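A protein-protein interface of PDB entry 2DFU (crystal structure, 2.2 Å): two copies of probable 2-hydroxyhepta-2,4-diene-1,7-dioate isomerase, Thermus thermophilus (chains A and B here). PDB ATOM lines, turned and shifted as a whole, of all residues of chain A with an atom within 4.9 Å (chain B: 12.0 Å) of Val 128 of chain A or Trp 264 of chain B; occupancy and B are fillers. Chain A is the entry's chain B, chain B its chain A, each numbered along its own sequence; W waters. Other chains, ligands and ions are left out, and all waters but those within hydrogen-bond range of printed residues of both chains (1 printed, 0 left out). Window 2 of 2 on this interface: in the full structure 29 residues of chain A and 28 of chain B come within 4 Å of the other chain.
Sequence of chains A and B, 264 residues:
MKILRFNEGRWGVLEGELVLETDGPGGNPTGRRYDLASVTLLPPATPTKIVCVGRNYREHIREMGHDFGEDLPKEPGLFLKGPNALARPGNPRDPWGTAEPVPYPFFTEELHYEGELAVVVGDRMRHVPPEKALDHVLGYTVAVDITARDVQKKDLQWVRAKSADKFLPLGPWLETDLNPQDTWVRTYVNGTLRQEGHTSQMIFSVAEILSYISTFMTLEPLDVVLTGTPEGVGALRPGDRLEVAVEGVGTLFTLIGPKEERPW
A ring nitrogen (ND1) of His 127 of chain A sits at hydrogen-bond distance from the guanidinium group of Arg 126 of chain A (3.4 Å). N of His 127 of chain A sits at hydrogen-bond distance from O of Ser 214 of chain A. NE2 of His 127 of chain A lies within hydrogen-bond range of O of Thr 215 of chain A (3.3 Å). OG of Ser 211 of chain A sits at hydrogen-bond distance from O of Val 128 of chain A, at 2.6 Å. The side-chain hydroxyl (OG) of Ser 214 of chain A lies within hydrogen-bond range of the backbone NH (N) of Val 128 of chain A (2.9 Å). The side-chain hydroxyl (OG) of Ser 214 of chain A lies within hydrogen-bond range of the backbone carbonyl oxygen (O) of Ser 211 of chain A, 2.6 Å away.
Among the printed residues, pairs that only touch across the chains: His 127 of chain A with Pro 263 of chain B (3.8 Å), His 127 of chain A with Trp 264 of chain B (3.8 Å), Val 128 of chain A with Trp 264 of chain B (3.5 Å), Ser 211 of chain A with Trp 264 of chain B (3.0 Å) and Thr 215 of chain A with Trp 264 of chain B (3.5 Å).
Val 128 of chain A touches just one residue of chain B: Trp 264. Of the printed residues of chain A, Trp 264 of chain B touches His 127, Val 128, Ser 211 and Thr 215. Pro 129 of chain A touches none of the printed residues of chain B. No residue of chain B comes within 4 Å of Lys 132 of chain A. Ala 133 of chain A touches none of the printed residues of chain B. Ser 211 of chain A touches just one residue of chain B: Trp 264. Ser 214 of chain A touches none of the printed residues of chain B. Printed residues of chain A within 4 Å of Pro 263 of chain B: His 127 (3.8 Å). The nearest printed residue of chain A that does not touch Trp 264 of chain B is Pro 130 of chain A (4.01 Å).
Along chain A the printed residues that touch a printed residue of chain B span positions 127 to 215. Among the printed residues, 5 pairs touch across the chains. Among the printed residues, no Asp or Glu carboxylate lies within 4 Å of a Lys or Arg side-chain nitrogen of the other chain.
No position is printed for both chains. Of the 5 pairs that touch across the chains among the printed residues, none has its exchanged pair printed and touching as well.
Water W1 bridges the side-chain carboxylate (OD2) of Asp 165 of chain B (3.0 Å) and the backbone carbonyl oxygen (O) of Ser 214 of chain A (3.0 Å).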
ATOM      1  N   MET A 125      -2.895  16.595  19.277  1.00  0.00           N
ATOM      2  CA  MET A 125      -3.563  17.065  18.069  1.00  0.00           C
ATOM      3  C   MET A 125      -3.795  15.984  17.024  1.00  0.00           C
ATOM      4  O   MET A 125      -2.847  15.416  16.485  1.00  0.00           O
ATOM      5  CB  MET A 125      -2.754  18.186  17.414  1.00  0.00           C
ATOM      6  CG  MET A 125      -2.488  19.379  18.307  1.00  0.00           C
ATOM      7  SD  MET A 125      -1.568  20.625  17.422  1.00  0.00           S
ATOM      8  CE  MET A 125      -2.929  21.423  16.477  1.00  0.00           C
ATOM      9  N   ARG A 126      -5.062  15.715  16.735  1.00  0.00           N
ATOM     10  CA  ARG A 126      -5.440  14.736  15.722  1.00  0.00           C
ATOM     11  C   ARG A 126      -6.672  15.297  15.023  1.00  0.00           C
ATOM     12  O   ARG A 126      -7.681  15.567  15.671  1.00  0.00           O
ATOM     13  CB  ARG A 126      -5.772  13.381  16.357  1.00  0.00           C
ATOM     14  CG  ARG A 126      -6.272  12.337  15.354  1.00  0.00           C
ATOM     15  CD  ARG A 126      -6.618  11.024  16.044  1.00  0.00           C
ATOM     16  NE  ARG A 126      -7.188  10.044  15.123  1.00  0.00           N
ATOM     17  CZ  ARG A 126      -8.457  10.032  14.717  1.00  0.00           C
ATOM     18  NH1 ARG A 126      -9.313  10.951  15.152  1.00  0.00           N
ATOM     19  NH2 ARG A 126      -8.872   9.101  13.866  1.00  0.00           N
ATOM     20  N   HIS A 127      -6.582  15.480  13.709  1.00  0.00           N
ATOM     21  CA  HIS A 127      -7.688  16.023  12.924  1.00  0.00           C
ATOM     22  C   HIS A 127      -8.168  17.340  13.529  1.00  0.00           C
ATOM     23  O   HIS A 127      -9.330  17.476  13.904  1.00  0.00           O
ATOM     24  CB  HIS A 127      -8.849  15.018  12.873  1.00  0.00           C
ATOM     25  CG  HIS A 127      -8.497  13.712  12.226  1.00  0.00           C
ATOM     26  ND1 HIS A 127      -9.351  12.629  12.222  1.00  0.00           N
ATOM     27  CD2 HIS A 127      -7.381  13.311  11.570  1.00  0.00           C
ATOM     28  CE1 HIS A 127      -8.776  11.618  11.595  1.00  0.00           C
ATOM     29  NE2 HIS A 127      -7.580  12.005  11.189  1.00  0.00           N
ATOM     30  N   VAL A 128      -7.261  18.305  13.633  1.00  0.00           N
ATOM     31  CA  VAL A 128      -7.587  19.612  14.195  1.00  0.00           C
ATOM     32  C   VAL A 128      -7.646  20.645  13.077  1.00  0.00           C
ATOM     33  O   VAL A 128      -6.679  20.821  12.336  1.00  0.00           O
ATOM     34  CB  VAL A 128      -6.520  20.073  15.226  1.00  0.00           C
ATOM     35  CG1 VAL A 128      -6.841  21.470  15.733  1.00  0.00           C
ATOM     36  CG2 VAL A 128      -6.449  19.091  16.384  1.00  0.00           C
ATOM     37  N   PRO A 129      -8.793  21.330  12.929  1.00  0.00           N
ATOM     38  CA  PRO A 129      -8.919  22.346  11.877  1.00  0.00           C
ATOM     39  C   PRO A 129      -8.014  23.549  12.167  1.00  0.00           C
ATOM     40  O   PRO A 129      -7.716  23.846  13.327  1.00  0.00           O
ATOM     41  CB  PRO A 129     -10.406  22.697  11.912  1.00  0.00           C
ATOM     42  CG  PRO A 129     -10.770  22.474  13.349  1.00  0.00           C
ATOM     43  CD  PRO A 129     -10.060  21.174  13.663  1.00  0.00           C
ATOM     44  N   PRO A 130      -7.568  24.253  11.115  1.00  0.00           N
ATOM     45  CA  PRO A 130      -6.691  25.422  11.256  1.00  0.00           C
ATOM     46  C   PRO A 130      -7.130  26.419  12.324  1.00  0.00           C
ATOM     47  O   PRO A 130      -6.314  26.875  13.128  1.00  0.00           O
ATOM     48  CB  PRO A 130      -6.706  26.039   9.859  1.00  0.00           C
ATOM     49  CG  PRO A 130      -6.878  24.845   8.970  1.00  0.00           C
ATOM     50  CD  PRO A 130      -7.938  24.047   9.703  1.00  0.00           C
ATOM     51  N   LYS A 132      -8.572  26.028  15.000  1.00  0.00           N
ATOM     52  CA  LYS A 132      -8.448  25.563  16.376  1.00  0.00           C
ATOM     53  C   LYS A 132      -7.033  25.118  16.704  1.00  0.00           C
ATOM     54  O   LYS A 132      -6.749  24.733  17.835  1.00  0.00           O
ATOM     55  CB  LYS A 132      -9.407  24.400  16.632  1.00  0.00           C
ATOM     56  CG  LYS A 132     -10.874  24.788  16.632  1.00  0.00           C
ATOM     57  CD  LYS A 132     -11.745  23.601  17.005  1.00  0.00           C
ATOM     58  CE  LYS A 132     -13.228  23.960  16.969  1.00  0.00           C
ATOM     59  NZ  LYS A 132     -14.095  22.800  17.329  1.00  0.00           N
ATOM     60  N   ALA A 133      -6.147  25.193  15.717  1.00  0.00           N
ATOM     61  CA  ALA A 133      -4.766  24.756  15.878  1.00  0.00           C
ATOM     62  C   ALA A 133      -3.930  25.474  16.934  1.00  0.00           C
ATOM     63  O   ALA A 133      -3.291  24.826  17.758  1.00  0.00           O
ATOM     64  CB  ALA A 133      -4.052  24.807  14.529  1.00  0.00           C
ATOM     65  N   HIS A 136      -3.910  24.576  20.710  1.00  0.00           N
ATOM     66  CA  HIS A 136      -3.199  23.393  21.193  1.00  0.00           C
ATOM     67  C   HIS A 136      -1.705  23.672  21.381  1.00  0.00           C
ATOM     68  O   HIS A 136      -0.937  22.768  21.718  1.00  0.00           O
ATOM     69  CB  HIS A 136      -3.363  22.218  20.209  1.00  0.00           C
ATOM     70  CG  HIS A 136      -4.773  21.728  20.064  1.00  0.00           C
ATOM     71  ND1 HIS A 136      -5.755  22.454  19.425  1.00  0.00           N
ATOM     72  CD2 HIS A 136      -5.364  20.582  20.476  1.00  0.00           C
ATOM     73  CE1 HIS A 136      -6.890  21.776  19.448  1.00  0.00           C
ATOM     74  NE2 HIS A 136      -6.680  20.637  20.080  1.00  0.00           N
ATOM     75  N   SER A 211      -2.368  21.879  11.565  1.00  0.00           N
ATOM     76  CA  SER A 211      -3.617  21.286  11.118  1.00  0.00           C
ATOM     77  C   SER A 211      -3.362  20.192  10.089  1.00  0.00           C
ATOM     78  O   SER A 211      -3.911  19.092  10.176  1.00  0.00           O
ATOM     79  CB  SER A 211      -4.513  22.359  10.506  1.00  0.00           C
ATOM     80  OG  SER A 211      -5.739  21.796  10.085  1.00  0.00           O
ATOM     81  N   SER A 214      -1.858  17.054  11.608  1.00  0.00           N
ATOM     82  CA  SER A 214      -2.872  16.337  12.369  1.00  0.00           C
ATOM     83  C   SER A 214      -3.831  15.496  11.531  1.00  0.00           C
ATOM     84  O   SER A 214      -4.562  14.678  12.082  1.00  0.00           O
ATOM     85  CB  SER A 214      -3.695  17.316  13.209  1.00  0.00           C
ATOM     86  OG  SER A 214      -4.622  18.018  12.400  1.00  0.00           O
ATOM     87  N   THR A 215      -3.847  15.690  10.213  1.00  0.00           N
ATOM     88  CA  THR A 215      -4.756  14.912   9.372  1.00  0.00           C
ATOM     89  C   THR A 215      -4.342  13.451   9.229  1.00  0.00           C
ATOM     90  O   THR A 215      -5.180  12.586   8.984  1.00  0.00           O
ATOM     91  CB  THR A 215      -4.880  15.507   7.952  1.00  0.00           C
ATOM     92  OG1 THR A 215      -3.599  15.501   7.310  1.00  0.00           O
ATOM     93  CG2 THR A 215      -5.421  16.927   8.011  1.00  0.00           C
ATOM     94  N   PRO B 105      -6.091   4.867   5.326  1.00  0.00           N
ATOM     95  CA  PRO B 105      -6.136   6.327   5.213  1.00  0.00           C
ATOM     96  C   PRO B 105      -6.913   6.933   4.057  1.00  0.00           C
ATOM     97  O   PRO B 105      -7.076   6.327   3.001  1.00  0.00           O
ATOM     98  CB  PRO B 105      -4.660   6.719   5.165  1.00  0.00           C
ATOM     99  CG  PRO B 105      -3.970   5.572   5.821  1.00  0.00           C
ATOM    100  CD  PRO B 105      -4.701   4.400   5.246  1.00  0.00           C
ATOM    101  N   PHE B 106      -7.374   8.157   4.279  1.00  0.00           N
ATOM    102  CA  PHE B 106      -8.121   8.890   3.278  1.00  0.00           C
ATOM    103  C   PHE B 106      -7.183   9.450   2.223  1.00  0.00           C
ATOM    104  O   PHE B 106      -7.552   9.540   1.056  1.00  0.00           O
ATOM    105  CB  PHE B 106      -8.888  10.042   3.931  1.00  0.00           C
ATOM    106  CG  PHE B 106      -9.542  10.968   2.942  1.00  0.00           C
ATOM    107  CD1 PHE B 106     -10.551  10.509   2.098  1.00  0.00           C
ATOM    108  CD2 PHE B 106      -9.128  12.294   2.832  1.00  0.00           C
ATOM    109  CE1 PHE B 106     -11.138  11.357   1.157  1.00  0.00           C
ATOM    110  CE2 PHE B 106      -9.708  13.149   1.893  1.00  0.00           C
ATOM    111  CZ  PHE B 106     -10.713  12.680   1.054  1.00  0.00           C
ATOM    112  N   PHE B 107      -5.966   9.807   2.637  1.00  0.00           N
ATOM    113  CA  PHE B 107      -4.977  10.406   1.737  1.00  0.00           C
ATOM    114  C   PHE B 107      -4.282   9.482   0.738  1.00  0.00           C
ATOM    115  O   PHE B 107      -3.496   9.942  -0.095  1.00  0.00           O
ATOM    116  CB  PHE B 107      -3.912  11.157   2.556  1.00  0.00           C
ATOM    117  CG  PHE B 107      -3.024  10.258   3.390  1.00  0.00           C
ATOM    118  CD1 PHE B 107      -1.962   9.565   2.807  1.00  0.00           C
ATOM    119  CD2 PHE B 107      -3.254  10.104   4.757  1.00  0.00           C
ATOM    120  CE1 PHE B 107      -1.140   8.729   3.574  1.00  0.00           C
ATOM    121  CE2 PHE B 107      -2.440   9.272   5.528  1.00  0.00           C
ATOM    122  CZ  PHE B 107      -1.381   8.583   4.934  1.00  0.00           C
ATOM    123  N   ARG B 160       4.198  11.053   5.459  1.00  0.00           N
ATOM    124  CA  ARG B 160       2.908  10.391   5.573  1.00  0.00           C
ATOM    125  C   ARG B 160       2.901   9.045   4.865  1.00  0.00           C
ATOM    126  O   ARG B 160       2.003   8.236   5.073  1.00  0.00           O
ATOM    127  CB  ARG B 160       1.747  11.279   5.099  1.00  0.00           C
ATOM    128  CG  ARG B 160       1.812  11.785   3.705  1.00  0.00           C
ATOM    129  CD  ARG B 160       0.605  12.674   3.432  1.00  0.00           C
ATOM    130  NE  ARG B 160       0.710  13.265   2.109  1.00  0.00           N
ATOM    131  CZ  ARG B 160      -0.301  13.801   1.438  1.00  0.00           C
ATOM    132  NH1 ARG B 160      -1.520  13.831   1.962  1.00  0.00           N
ATOM    133  NH2 ARG B 160      -0.088  14.299   0.229  1.00  0.00           N
ATOM    134  N   ASP B 165      -0.282   7.629  11.461  1.00  0.00           N
ATOM    135  CA  ASP B 165      -0.695   6.890  12.651  1.00  0.00           C
ATOM    136  C   ASP B 165      -0.943   5.408  12.344  1.00  0.00           C
ATOM    137  O   ASP B 165      -1.530   5.074  11.320  1.00  0.00           O
ATOM    138  CB  ASP B 165      -1.972   7.496  13.252  1.00  0.00           C
ATOM    139  CG  ASP B 165      -1.732   8.854  13.903  1.00  0.00           C
ATOM    140  OD1 ASP B 165      -0.563   9.202  14.175  1.00  0.00           O
ATOM    141  OD2 ASP B 165      -2.720   9.569  14.159  1.00  0.00           O
ATOM    142  N   LYS B 259     -11.865   2.061   5.282  1.00  0.00           N
ATOM    143  CA  LYS B 259     -11.241   3.246   4.712  1.00  0.00           C
ATOM    144  C   LYS B 259     -11.817   4.471   5.395  1.00  0.00           C
ATOM    145  O   LYS B 259     -13.021   4.558   5.608  1.00  0.00           O
ATOM    146  CB  LYS B 259     -11.488   3.358   3.204  1.00  0.00           C
ATOM    147  CG  LYS B 259     -10.416   4.217   2.519  1.00  0.00           C
ATOM    148  CD  LYS B 259     -11.004   5.255   1.588  1.00  0.00           C
ATOM    149  CE  LYS B 259      -9.977   6.336   1.239  1.00  0.00           C
ATOM    150  NZ  LYS B 259      -8.741   5.800   0.617  1.00  0.00           N
ATOM    151  N   GLU B 260     -10.952   5.413   5.747  1.00  0.00           N
ATOM    152  CA  GLU B 260     -11.387   6.635   6.407  1.00  0.00           C
ATOM    153  C   GLU B 260     -11.870   7.640   5.365  1.00  0.00           C
ATOM    154  O   GLU B 260     -11.531   7.535   4.191  1.00  0.00           O
ATOM    155  CB  GLU B 260     -10.233   7.241   7.211  1.00  0.00           C
ATOM    156  CG  GLU B 260      -9.645   6.300   8.254  1.00  0.00           C
ATOM    157  CD  GLU B 260      -8.651   6.990   9.181  1.00  0.00           C
ATOM    158  OE1 GLU B 260      -7.684   7.602   8.676  1.00  0.00           O
ATOM    159  OE2 GLU B 260      -8.836   6.917  10.419  1.00  0.00           O
ATOM    160  N   GLU B 261     -12.670   8.607   5.793  1.00  0.00           N
ATOM    161  CA  GLU B 261     -13.165   9.626   4.878  1.00  0.00           C
ATOM    162  C   GLU B 261     -12.545  10.963   5.261  1.00  0.00           C
ATOM    163  O   GLU B 261     -11.699  11.008   6.150  1.00  0.00           O
ATOM    164  CB  GLU B 261     -14.699   9.659   4.905  1.00  0.00           C
ATOM    165  CG  GLU B 261     -15.316   9.694   6.293  1.00  0.00           C
ATOM    166  CD  GLU B 261     -16.791   9.317   6.280  1.00  0.00           C
ATOM    167  OE1 GLU B 261     -17.548   9.895   5.471  1.00  0.00           O
ATOM    168  OE2 GLU B 261     -17.195   8.445   7.081  1.00  0.00           O
ATOM    169  N   ARG B 262     -12.945  12.036   4.583  1.00  0.00           N
ATOM    170  CA  ARG B 262     -12.445  13.390   4.870  1.00  0.00           C
ATOM    171  C   ARG B 262     -12.211  13.660   6.377  1.00  0.00           C
ATOM    172  O   ARG B 262     -13.047  13.430   7.226  1.00  0.00           O
ATOM    173  CB  ARG B 262     -13.467  14.410   4.347  1.00  0.00           C
ATOM    174  CG  ARG B 262     -13.373  14.626   2.834  1.00  0.00           C
ATOM    175  CD  ARG B 262     -13.943  13.438   2.049  1.00  0.00           C
ATOM    176  NE  ARG B 262     -14.579  13.867   0.796  1.00  0.00           N
ATOM    177  CZ  ARG B 262     -13.829  14.522  -0.108  1.00  0.00           C
ATOM    178  NH1 ARG B 262     -12.564  14.812   0.159  1.00  0.00           N
ATOM    179  NH2 ARG B 262     -14.345  14.824  -1.302  1.00  0.00           N
ATOM    180  N   PRO B 263     -10.975  14.143   6.650  1.00  0.00           N
ATOM    181  CA  PRO B 263     -10.466  14.386   8.012  1.00  0.00           C
ATOM    182  C   PRO B 263     -11.441  15.124   8.923  1.00  0.00           C
ATOM    183  O   PRO B 263     -11.491  14.948  10.136  1.00  0.00           O
ATOM    184  CB  PRO B 263      -9.197  15.229   7.879  1.00  0.00           C
ATOM    185  CG  PRO B 263      -9.022  15.609   6.409  1.00  0.00           C
ATOM    186  CD  PRO B 263     -10.002  14.577   5.686  1.00  0.00           C
ATOM    187  N   TRP B 264     -12.168  16.035   8.298  1.00  0.00           N
ATOM    188  CA  TRP B 264     -13.196  16.753   9.027  1.00  0.00           C
ATOM    189  C   TRP B 264     -14.114  17.455   8.045  1.00  0.00           C
ATOM    190  O   TRP B 264     -15.275  17.702   8.292  1.00  0.00           O
ATOM    191  CB  TRP B 264     -12.519  17.738   9.999  1.00  0.00           C
ATOM    192  CG  TRP B 264     -11.691  18.745   9.281  1.00  0.00           C
ATOM    193  CD1 TRP B 264     -12.170  19.724   8.390  1.00  0.00           C
ATOM    194  CD2 TRP B 264     -10.238  18.912   9.333  1.00  0.00           C
ATOM    195  NE1 TRP B 264     -11.177  20.481   7.861  1.00  0.00           N
ATOM    196  CE2 TRP B 264      -9.916  19.973   8.445  1.00  0.00           C
ATOM    197  CE3 TRP B 264      -9.203  18.271  10.020  1.00  0.00           C
ATOM    198  CZ2 TRP B 264      -8.597  20.361   8.265  1.00  0.00           C
ATOM    199  CZ3 TRP B 264      -7.883  18.661   9.840  1.00  0.00           C
ATOM    200  CH2 TRP B 264      -7.579  19.708   8.951  1.00  0.00           C
ATOM    201  OXT TRP B 264     -13.749  17.815   6.946  1.00  0.00           O
HETATM  202  O   HOH W   1      -3.937  11.798  12.605  1.00  0.00           O
